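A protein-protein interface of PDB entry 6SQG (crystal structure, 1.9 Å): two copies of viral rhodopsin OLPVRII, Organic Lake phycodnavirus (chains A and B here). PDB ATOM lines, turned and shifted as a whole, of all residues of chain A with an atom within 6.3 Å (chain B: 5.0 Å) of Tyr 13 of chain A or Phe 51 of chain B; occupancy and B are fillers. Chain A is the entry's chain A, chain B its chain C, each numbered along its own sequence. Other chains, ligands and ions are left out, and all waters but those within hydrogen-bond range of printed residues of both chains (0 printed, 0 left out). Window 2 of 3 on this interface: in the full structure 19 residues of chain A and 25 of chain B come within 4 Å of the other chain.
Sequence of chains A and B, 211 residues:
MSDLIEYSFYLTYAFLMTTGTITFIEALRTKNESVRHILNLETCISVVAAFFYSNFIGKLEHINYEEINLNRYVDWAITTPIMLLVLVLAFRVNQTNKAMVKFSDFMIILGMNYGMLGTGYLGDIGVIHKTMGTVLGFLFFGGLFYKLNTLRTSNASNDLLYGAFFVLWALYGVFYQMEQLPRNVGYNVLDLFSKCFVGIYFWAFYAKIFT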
ATOM      1  N   SER A   8     -16.576  -0.334 -20.838  1.00  0.00           N
ATOM      2  CA  SER A   8     -15.933   0.095 -19.600  1.00  0.00           C
ATOM      3  C   SER A   8     -15.226   1.441 -19.788  1.00  0.00           C
ATOM      4  O   SER A   8     -15.179   2.242 -18.858  1.00  0.00           O
ATOM      5  CB  SER A   8     -14.972  -0.980 -19.047  1.00  0.00           C
ATOM      6  OG  SER A   8     -13.856  -1.186 -19.894  1.00  0.00           O
ATOM      7  N   PHE A   9     -14.699   1.691 -20.982  1.00  0.00           N
ATOM      8  CA  PHE A   9     -14.111   3.001 -21.301  1.00  0.00           C
ATOM      9  C   PHE A   9     -15.185   4.088 -21.232  1.00  0.00           C
ATOM     10  O   PHE A   9     -14.977   5.156 -20.650  1.00  0.00           O
ATOM     11  CB  PHE A   9     -13.472   3.000 -22.692  1.00  0.00           C
ATOM     12  CG  PHE A   9     -12.033   2.541 -22.716  1.00  0.00           C
ATOM     13  CD1 PHE A   9     -11.064   3.213 -22.002  1.00  0.00           C
ATOM     14  CD2 PHE A   9     -11.653   1.451 -23.480  1.00  0.00           C
ATOM     15  CE1 PHE A   9      -9.742   2.800 -22.033  1.00  0.00           C
ATOM     16  CE2 PHE A   9     -10.332   1.035 -23.515  1.00  0.00           C
ATOM     17  CZ  PHE A   9      -9.376   1.712 -22.791  1.00  0.00           C
ATOM     18  N   TYR A  10     -16.339   3.810 -21.834  1.00  0.00           N
ATOM     19  CA  TYR A  10     -17.416   4.790 -21.898  1.00  0.00           C
ATOM     20  C   TYR A  10     -18.023   5.041 -20.543  1.00  0.00           C
ATOM     21  O   TYR A  10     -18.382   6.167 -20.213  1.00  0.00           O
ATOM     22  CB  TYR A  10     -18.490   4.362 -22.896  1.00  0.00           C
ATOM     23  CG  TYR A  10     -18.141   4.741 -24.307  1.00  0.00           C
ATOM     24  CD1 TYR A  10     -18.478   5.987 -24.807  1.00  0.00           C
ATOM     25  CD2 TYR A  10     -17.453   3.867 -25.135  1.00  0.00           C
ATOM     26  CE1 TYR A  10     -18.155   6.350 -26.096  1.00  0.00           C
ATOM     27  CE2 TYR A  10     -17.128   4.220 -26.431  1.00  0.00           C
ATOM     28  CZ  TYR A  10     -17.484   5.466 -26.904  1.00  0.00           C
ATOM     29  OH  TYR A  10     -17.168   5.847 -28.185  1.00  0.00           O
ATOM     30  N   LEU A  11     -18.132   3.987 -19.752  1.00  0.00           N
ATOM     31  CA  LEU A  11     -18.668   4.113 -18.412  1.00  0.00           C
ATOM     32  C   LEU A  11     -17.825   5.076 -17.583  1.00  0.00           C
ATOM     33  O   LEU A  11     -18.343   5.978 -16.939  1.00  0.00           O
ATOM     34  CB  LEU A  11     -18.714   2.743 -17.741  1.00  0.00           C
ATOM     35  CG  LEU A  11     -19.209   2.691 -16.300  1.00  0.00           C
ATOM     36  CD1 LEU A  11     -20.640   3.212 -16.192  1.00  0.00           C
ATOM     37  CD2 LEU A  11     -19.123   1.274 -15.751  1.00  0.00           C
ATOM     38  N   THR A  12     -16.514   4.868 -17.580  1.00  0.00           N
ATOM     39  CA  THR A  12     -15.635   5.690 -16.763  1.00  0.00           C
ATOM     40  C   THR A  12     -15.593   7.109 -17.323  1.00  0.00           C
ATOM     41  O   THR A  12     -15.693   8.093 -16.583  1.00  0.00           O
ATOM     42  CB  THR A  12     -14.250   5.034 -16.648  1.00  0.00           C
ATOM     43  OG1 THR A  12     -14.386   3.803 -15.927  1.00  0.00           O
ATOM     44  CG2 THR A  12     -13.250   5.936 -15.924  1.00  0.00           C
ATOM     45  N   TYR A  13     -15.496   7.225 -18.636  1.00  0.00           N
ATOM     46  CA  TYR A  13     -15.453   8.540 -19.258  1.00  0.00           C
ATOM     47  C   TYR A  13     -16.684   9.349 -18.870  1.00  0.00           C
ATOM     48  O   TYR A  13     -16.575  10.516 -18.459  1.00  0.00           O
ATOM     49  CB  TYR A  13     -15.360   8.390 -20.774  1.00  0.00           C
ATOM     50  CG  TYR A  13     -15.263   9.690 -21.540  1.00  0.00           C
ATOM     51  CD1 TYR A  13     -14.450  10.728 -21.097  1.00  0.00           C
ATOM     52  CD2 TYR A  13     -15.948   9.857 -22.740  1.00  0.00           C
ATOM     53  CE1 TYR A  13     -14.339  11.911 -21.820  1.00  0.00           C
ATOM     54  CE2 TYR A  13     -15.850  11.034 -23.465  1.00  0.00           C
ATOM     55  CZ  TYR A  13     -15.051  12.056 -22.999  1.00  0.00           C
ATOM     56  OH  TYR A  13     -14.964  13.219 -23.721  1.00  0.00           O
ATOM     57  N   ALA A  14     -17.861   8.726 -18.971  1.00  0.00           N
ATOM     58  CA  ALA A  14     -19.110   9.419 -18.678  1.00  0.00           C
ATOM     59  C   ALA A  14     -19.209   9.756 -17.191  1.00  0.00           C
ATOM     60  O   ALA A  14     -19.685  10.829 -16.820  1.00  0.00           O
ATOM     61  CB  ALA A  14     -20.311   8.592 -19.131  1.00  0.00           C
ATOM     62  N   PHE A  15     -18.753   8.857 -16.327  1.00  0.00           N
ATOM     63  CA  PHE A  15     -18.796   9.156 -14.897  1.00  0.00           C
ATOM     64  C   PHE A  15     -17.782  10.240 -14.508  1.00  0.00           C
ATOM     65  O   PHE A  15     -17.996  10.969 -13.540  1.00  0.00           O
ATOM     66  CB  PHE A  15     -18.625   7.885 -14.043  1.00  0.00           C
ATOM     67  CG  PHE A  15     -19.852   7.515 -13.244  1.00  0.00           C
ATOM     68  CD1 PHE A  15     -20.352   8.383 -12.275  1.00  0.00           C
ATOM     69  CD2 PHE A  15     -20.486   6.299 -13.432  1.00  0.00           C
ATOM     70  CE1 PHE A  15     -21.473   8.055 -11.532  1.00  0.00           C
ATOM     71  CE2 PHE A  15     -21.610   5.966 -12.695  1.00  0.00           C
ATOM     72  CZ  PHE A  15     -22.102   6.838 -11.742  1.00  0.00           C
ATOM     73  N   LEU A  16     -16.692  10.371 -15.261  1.00  0.00           N
ATOM     74  CA  LEU A  16     -15.749  11.465 -15.004  1.00  0.00           C
ATOM     75  C   LEU A  16     -16.391  12.829 -15.332  1.00  0.00           C
ATOM     76  O   LEU A  16     -16.130  13.829 -14.654  1.00  0.00           O
ATOM     77  CB  LEU A  16     -14.458  11.274 -15.793  1.00  0.00           C
ATOM     78  CG  LEU A  16     -13.532  10.156 -15.289  1.00  0.00           C
ATOM     79  CD1 LEU A  16     -12.557   9.731 -16.368  1.00  0.00           C
ATOM     80  CD2 LEU A  16     -12.792  10.607 -14.040  1.00  0.00           C
ATOM     81  N   MET A  17     -17.222  12.868 -16.370  1.00  0.00           N
ATOM     82  CA  MET A  17     -17.987  14.075 -16.685  1.00  0.00           C
ATOM     83  C   MET A  17     -18.915  14.429 -15.531  1.00  0.00           C
ATOM     84  O   MET A  17     -19.050  15.590 -15.173  1.00  0.00           O
ATOM     85  CB  MET A  17     -18.820  13.879 -17.946  1.00  0.00           C
ATOM     86  CG  MET A  17     -18.007  13.646 -19.204  1.00  0.00           C
ATOM     87  SD  MET A  17     -19.068  13.460 -20.654  1.00  0.00           S
ATOM     88  CE  MET A  17     -17.957  12.538 -21.717  1.00  0.00           C
ATOM     89  N   THR A  18     -19.554  13.419 -14.960  1.00  0.00           N
ATOM     90  CA  THR A  18     -20.455  13.602 -13.840  1.00  0.00           C
ATOM     91  C   THR A  18     -19.726  14.160 -12.638  1.00  0.00           C
ATOM     92  O   THR A  18     -20.147  15.152 -12.043  1.00  0.00           O
ATOM     93  CB  THR A  18     -21.102  12.257 -13.444  1.00  0.00           C
ATOM     94  OG1 THR A  18     -21.952  11.816 -14.507  1.00  0.00           O
ATOM     95  CG2 THR A  18     -21.927  12.404 -12.178  1.00  0.00           C
ATOM     96  N   ALA A  49      -8.286  13.162 -16.252  1.00  0.00           N
ATOM     97  CA  ALA A  49      -8.685  11.794 -16.579  1.00  0.00           C
ATOM     98  C   ALA A  49      -9.659  11.752 -17.767  1.00  0.00           C
ATOM     99  O   ALA A  49      -9.525  10.896 -18.666  1.00  0.00           O
ATOM    100  CB  ALA A  49      -9.287  11.101 -15.365  1.00  0.00           C
ATOM    101  N   ALA A  50     -10.633  12.665 -17.782  1.00  0.00           N
ATOM    102  CA  ALA A  50     -11.584  12.721 -18.881  1.00  0.00           C
ATOM    103  C   ALA A  50     -10.848  12.945 -20.197  1.00  0.00           C
ATOM    104  O   ALA A  50     -11.175  12.328 -21.208  1.00  0.00           O
ATOM    105  CB  ALA A  50     -12.630  13.802 -18.668  1.00  0.00           C
ATOM    106  N   PHE A  51      -9.841  13.811 -20.188  1.00  0.00           N
ATOM    107  CA  PHE A  51      -9.051  14.020 -21.393  1.00  0.00           C
ATOM    108  C   PHE A  51      -8.401  12.721 -21.869  1.00  0.00           C
ATOM    109  O   PHE A  51      -8.428  12.402 -23.059  1.00  0.00           O
ATOM    110  CB  PHE A  51      -7.977  15.091 -21.193  1.00  0.00           C
ATOM    111  CG  PHE A  51      -6.923  15.062 -22.250  1.00  0.00           C
ATOM    112  CD1 PHE A  51      -7.229  15.424 -23.549  1.00  0.00           C
ATOM    113  CD2 PHE A  51      -5.645  14.605 -21.969  1.00  0.00           C
ATOM    114  CE1 PHE A  51      -6.278  15.355 -24.551  1.00  0.00           C
ATOM    115  CE2 PHE A  51      -4.685  14.538 -22.971  1.00  0.00           C
ATOM    116  CZ  PHE A  51      -5.003  14.919 -24.259  1.00  0.00           C
ATOM    117  N   TYR A  53      -9.262   9.556 -21.110  1.00  0.00           N
ATOM    118  CA  TYR A  53     -10.269   8.604 -21.549  1.00  0.00           C
ATOM    119  C   TYR A  53     -10.819   8.939 -22.934  1.00  0.00           C
ATOM    120  O   TYR A  53     -11.044   8.037 -23.741  1.00  0.00           O
ATOM    121  CB  TYR A  53     -11.371   8.427 -20.511  1.00  0.00           C
ATOM    122  CG  TYR A  53     -10.977   7.359 -19.508  1.00  0.00           C
ATOM    123  CD1 TYR A  53     -10.091   7.642 -18.479  1.00  0.00           C
ATOM    124  CD2 TYR A  53     -11.462   6.060 -19.619  1.00  0.00           C
ATOM    125  CE1 TYR A  53      -9.712   6.671 -17.574  1.00  0.00           C
ATOM    126  CE2 TYR A  53     -11.090   5.075 -18.721  1.00  0.00           C
ATOM    127  CZ  TYR A  53     -10.216   5.381 -17.701  1.00  0.00           C
ATOM    128  OH  TYR A  53      -9.839   4.409 -16.810  1.00  0.00           O
ATOM    129  N   SER A  54     -11.010  10.222 -23.225  1.00  0.00           N
ATOM    130  CA  SER A  54     -11.503  10.621 -24.536  1.00  0.00           C
ATOM    131  C   SER A  54     -10.481  10.238 -25.602  1.00  0.00           C
ATOM    132  O   SER A  54     -10.844   9.799 -26.689  1.00  0.00           O
ATOM    133  CB  SER A  54     -11.798  12.122 -24.589  1.00  0.00           C
ATOM    134  OG  SER A  54     -10.607  12.886 -24.587  1.00  0.00           O
ATOM    135  N   ILE A  57     -10.474   6.399 -26.106  1.00  0.00           N
ATOM    136  CA  ILE A  57     -11.659   6.004 -26.848  1.00  0.00           C
ATOM    137  C   ILE A  57     -11.462   6.360 -28.322  1.00  0.00           C
ATOM    138  O   ILE A  57     -11.721   5.546 -29.195  1.00  0.00           O
ATOM    139  CB  ILE A  57     -12.921   6.685 -26.307  1.00  0.00           C
ATOM    140  CG1 ILE A  57     -13.286   6.108 -24.938  1.00  0.00           C
ATOM    141  CG2 ILE A  57     -14.083   6.508 -27.278  1.00  0.00           C
ATOM    142  CD1 ILE A  57     -14.294   6.940 -24.181  1.00  0.00           C
ATOM    143  N   SER B  46     -28.374  15.610 -17.275  1.00  0.00           N
ATOM    144  CA  SER B  46     -28.454  16.149 -18.626  1.00  0.00           C
ATOM    145  C   SER B  46     -27.123  16.057 -19.364  1.00  0.00           C
ATOM    146  O   SER B  46     -27.088  15.753 -20.551  1.00  0.00           O
ATOM    147  CB  SER B  46     -28.900  17.610 -18.594  1.00  0.00           C
ATOM    148  OG  SER B  46     -30.260  17.717 -18.261  1.00  0.00           O
ATOM    149  N   VAL B  47     -26.033  16.340 -18.662  1.00  0.00           N
ATOM    150  CA  VAL B  47     -24.709  16.231 -19.250  1.00  0.00           C
ATOM    151  C   VAL B  47     -24.428  14.822 -19.777  1.00  0.00           C
ATOM    152  O   VAL B  47     -23.993  14.641 -20.923  1.00  0.00           O
ATOM    153  CB  VAL B  47     -23.627  16.623 -18.231  1.00  0.00           C
ATOM    154  CG1 VAL B  47     -22.249  16.198 -18.721  1.00  0.00           C
ATOM    155  CG2 VAL B  47     -23.667  18.131 -17.970  1.00  0.00           C
ATOM    156  N   VAL B  48     -24.697  13.823 -18.951  1.00  0.00           N
ATOM    157  CA  VAL B  48     -24.413  12.432 -19.313  1.00  0.00           C
ATOM    158  C   VAL B  48     -25.300  11.930 -20.438  1.00  0.00           C
ATOM    159  O   VAL B  48     -24.820  11.326 -21.411  1.00  0.00           O
ATOM    160  CB  VAL B  48     -24.586  11.506 -18.105  1.00  0.00           C
ATOM    161  CG1 VAL B  48     -24.526  10.041 -18.549  1.00  0.00           C
ATOM    162  CG2 VAL B  48     -23.510  11.810 -17.077  1.00  0.00           C
ATOM    163  N   ALA B  49     -26.603  12.144 -20.298  1.00  0.00           N
ATOM    164  CA  ALA B  49     -27.532  11.705 -21.319  1.00  0.00           C
ATOM    165  C   ALA B  49     -27.250  12.411 -22.659  1.00  0.00           C
ATOM    166  O   ALA B  49     -27.276  11.772 -23.714  1.00  0.00           O
ATOM    167  CB  ALA B  49     -28.974  11.918 -20.861  1.00  0.00           C
ATOM    168  N   ALA B  50     -26.971  13.714 -22.624  1.00  0.00           N
ATOM    169  CA  ALA B  50     -26.606  14.455 -23.851  1.00  0.00           C
ATOM    170  C   ALA B  50     -25.410  13.853 -24.562  1.00  0.00           C
ATOM    171  O   ALA B  50     -25.369  13.795 -25.802  1.00  0.00           O
ATOM    172  CB  ALA B  50     -26.325  15.920 -23.539  1.00  0.00           C
ATOM    173  N   PHE B  51     -24.417  13.440 -23.783  1.00  0.00           N
ATOM    174  CA  PHE B  51     -23.254  12.787 -24.334  1.00  0.00           C
ATOM    175  C   PHE B  51     -23.640  11.511 -25.081  1.00  0.00           C
ATOM    176  O   PHE B  51     -23.233  11.312 -26.222  1.00  0.00           O
ATOM    177  CB  PHE B  51     -22.228  12.477 -23.239  1.00  0.00           C
ATOM    178  CG  PHE B  51     -21.137  11.556 -23.688  1.00  0.00           C
ATOM    179  CD1 PHE B  51     -20.193  11.981 -24.614  1.00  0.00           C
ATOM    180  CD2 PHE B  51     -21.046  10.265 -23.186  1.00  0.00           C
ATOM    181  CE1 PHE B  51     -19.186  11.135 -25.041  1.00  0.00           C
ATOM    182  CE2 PHE B  51     -20.040   9.413 -23.609  1.00  0.00           C
ATOM    183  CZ  PHE B  51     -19.109   9.848 -24.537  1.00  0.00           C
ATOM    184  N   PHE B  52     -24.418  10.640 -24.451  1.00  0.00           N
ATOM    185  CA  PHE B  52     -24.822   9.428 -25.141  1.00  0.00           C
ATOM    186  C   PHE B  52     -25.696   9.709 -26.360  1.00  0.00           C
ATOM    187  O   PHE B  52     -25.519   9.073 -27.393  1.00  0.00           O
ATOM    188  CB  PHE B  52     -25.439   8.406 -24.179  1.00  0.00           C
ATOM    189  CG  PHE B  52     -24.412   7.759 -23.294  1.00  0.00           C
ATOM    190  CD1 PHE B  52     -23.591   6.768 -23.788  1.00  0.00           C
ATOM    191  CD2 PHE B  52     -24.226   8.186 -21.991  1.00  0.00           C
ATOM    192  CE1 PHE B  52     -22.626   6.195 -22.995  1.00  0.00           C
ATOM    193  CE2 PHE B  52     -23.263   7.626 -21.196  1.00  0.00           C
ATOM    194  CZ  PHE B  52     -22.458   6.625 -21.696  1.00  0.00           C
ATOM    195  N   TYR B  53     -26.598  10.679 -26.271  1.00  0.00           N
ATOM    196  CA  TYR B  53     -27.386  11.048 -27.449  1.00  0.00           C
ATOM    197  C   TYR B  53     -26.518  11.595 -28.601  1.00  0.00           C
ATOM    198  O   TYR B  53     -26.762  11.251 -29.764  1.00  0.00           O
ATOM    199  CB  TYR B  53     -28.549  11.998 -27.096  1.00  0.00           C
ATOM    200  CG  TYR B  53     -29.770  11.234 -26.661  1.00  0.00           C
ATOM    201  CD1 TYR B  53     -29.868  10.725 -25.376  1.00  0.00           C
ATOM    202  CD2 TYR B  53     -30.805  10.970 -27.546  1.00  0.00           C
ATOM    203  CE1 TYR B  53     -30.969   9.992 -24.977  1.00  0.00           C
ATOM    204  CE2 TYR B  53     -31.908  10.237 -27.153  1.00  0.00           C
ATOM    205  CZ  TYR B  53     -31.982   9.752 -25.862  1.00  0.00           C
ATOM    206  OH  TYR B  53     -33.076   9.028 -25.445  1.00  0.00           O
ATOM    207  N   SER B  54     -25.500  12.406 -28.308  1.00  0.00           N
ATOM    208  CA  SER B  54     -24.623  12.881 -29.386  1.00  0.00           C
ATOM    209  C   SER B  54     -23.970  11.682 -30.058  1.00  0.00           C
ATOM    210  O   SER B  54     -23.797  11.657 -31.271  1.00  0.00           O
ATOM    211  CB  SER B  54     -23.529  13.830 -28.881  1.00  0.00           C
ATOM    212  OG  SER B  54     -22.676  13.176 -27.958  1.00  0.00           O
ATOM    213  N   ASN B  55     -23.614  10.681 -29.261  1.00  0.00           N
ATOM    214  CA  ASN B  55     -23.033   9.451 -29.804  1.00  0.00           C
ATOM    215  C   ASN B  55     -24.010   8.668 -30.665  1.00  0.00           C
ATOM    216  O   ASN B  55     -23.675   8.274 -31.791  1.00  0.00           O
ATOM    217  CB  ASN B  55     -22.494   8.566 -28.690  1.00  0.00           C
ATOM    218  CG  ASN B  55     -21.062   8.887 -28.353  1.00  0.00           C
ATOM    219  OD1 ASN B  55     -20.784   9.830 -27.619  1.00  0.00           O
ATOM    220  ND2 ASN B  55     -20.137   8.105 -28.901  1.00  0.00           N
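Of the 10 printed residues of chain B, 4 touch a printed residue of chain A. Hydrophobic or aromatic side chains of chain B within 4 Å of the printed part of chain A: Val 48, Phe 51 and Phe 52. Among the printed residues, 7 pairs touch across the chains.
The backbone carbonyl oxygen of Ala 14 of chain A is in hydrogen-bond range of the side-chain hydroxyl of Thr 18 of chain A. The side-chain amide oxygen (OD1) of Asn 55 of chain B lies close to the backbone carbonyl oxygen (O) of Phe 51 of chain B (3.2 Å). The backbone carbonyl oxygen (O) of Phe 51 of chain B is in hydrogen-bond range of the side-chain hydroxyl (OG) of Ser 54 of chain B (2.6 Å).
Of the printed residues of chain B, Tyr 10 of chain A touches Phe 51 (3.9 Å) and Asn 55 (3.8 Å). Of chain B, only Phe 51 comes within 4 Å of Tyr 13 of chain A. Printed residues of chain B within 4 Å of Met 17 of chain A: Phe 51. Printed residues of chain A within 4 Å of Val 48 of chain B: Ala 14 (3.96 Å) and Thr 18 (3.0 Å). Of the printed residues of chain A, Phe 51 of chain B touches Tyr 10 (3.9 Å), Tyr 13 (3.6 Å) and Met 17 (3.7 Å). Tyr 53 of chain B touches none of the printed residues of chain A. Printed residues of chain A within 4 Å of Asn 55 of chain B: Tyr 10 (3.8 Å). The nearest printed residue of chain B that does not touch Tyr 13 of chain A is Asn 55 of chain B (6.6 Å). The nearest printed residue of chain B that does not touch Met 17 of chain A is Val 47 of chain B (4.2 Å).
CD1 of Tyr 10 of chain A touches CZ of Phe 51 of chain B, at 3.9 Å. Asn 55 of chain B touches Tyr 10 of chain A. Tyr 13 of chain A touches Phe 51 of chain B (CE2 to CZ, 3.6 Å). Val 48 of chain B touches Ala 14 of chain A. Phe 52 of chain B touches Ala 14 of chain A (CE2 to CB, 3.7 Å). CE of Met 17 of chain A touches CD1 of Phe 51 of chain B, 3.7 Å away. Val 48 of chain B touches Thr 18 of chain A (CG2 to OG1, 3.0 Å).
Positions printed for both chains: 49, 50, 51, 53 and 54. Of the 7 pairs that touch across the chains among the printed residues, none has its exchanged pair printed and touching as well.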
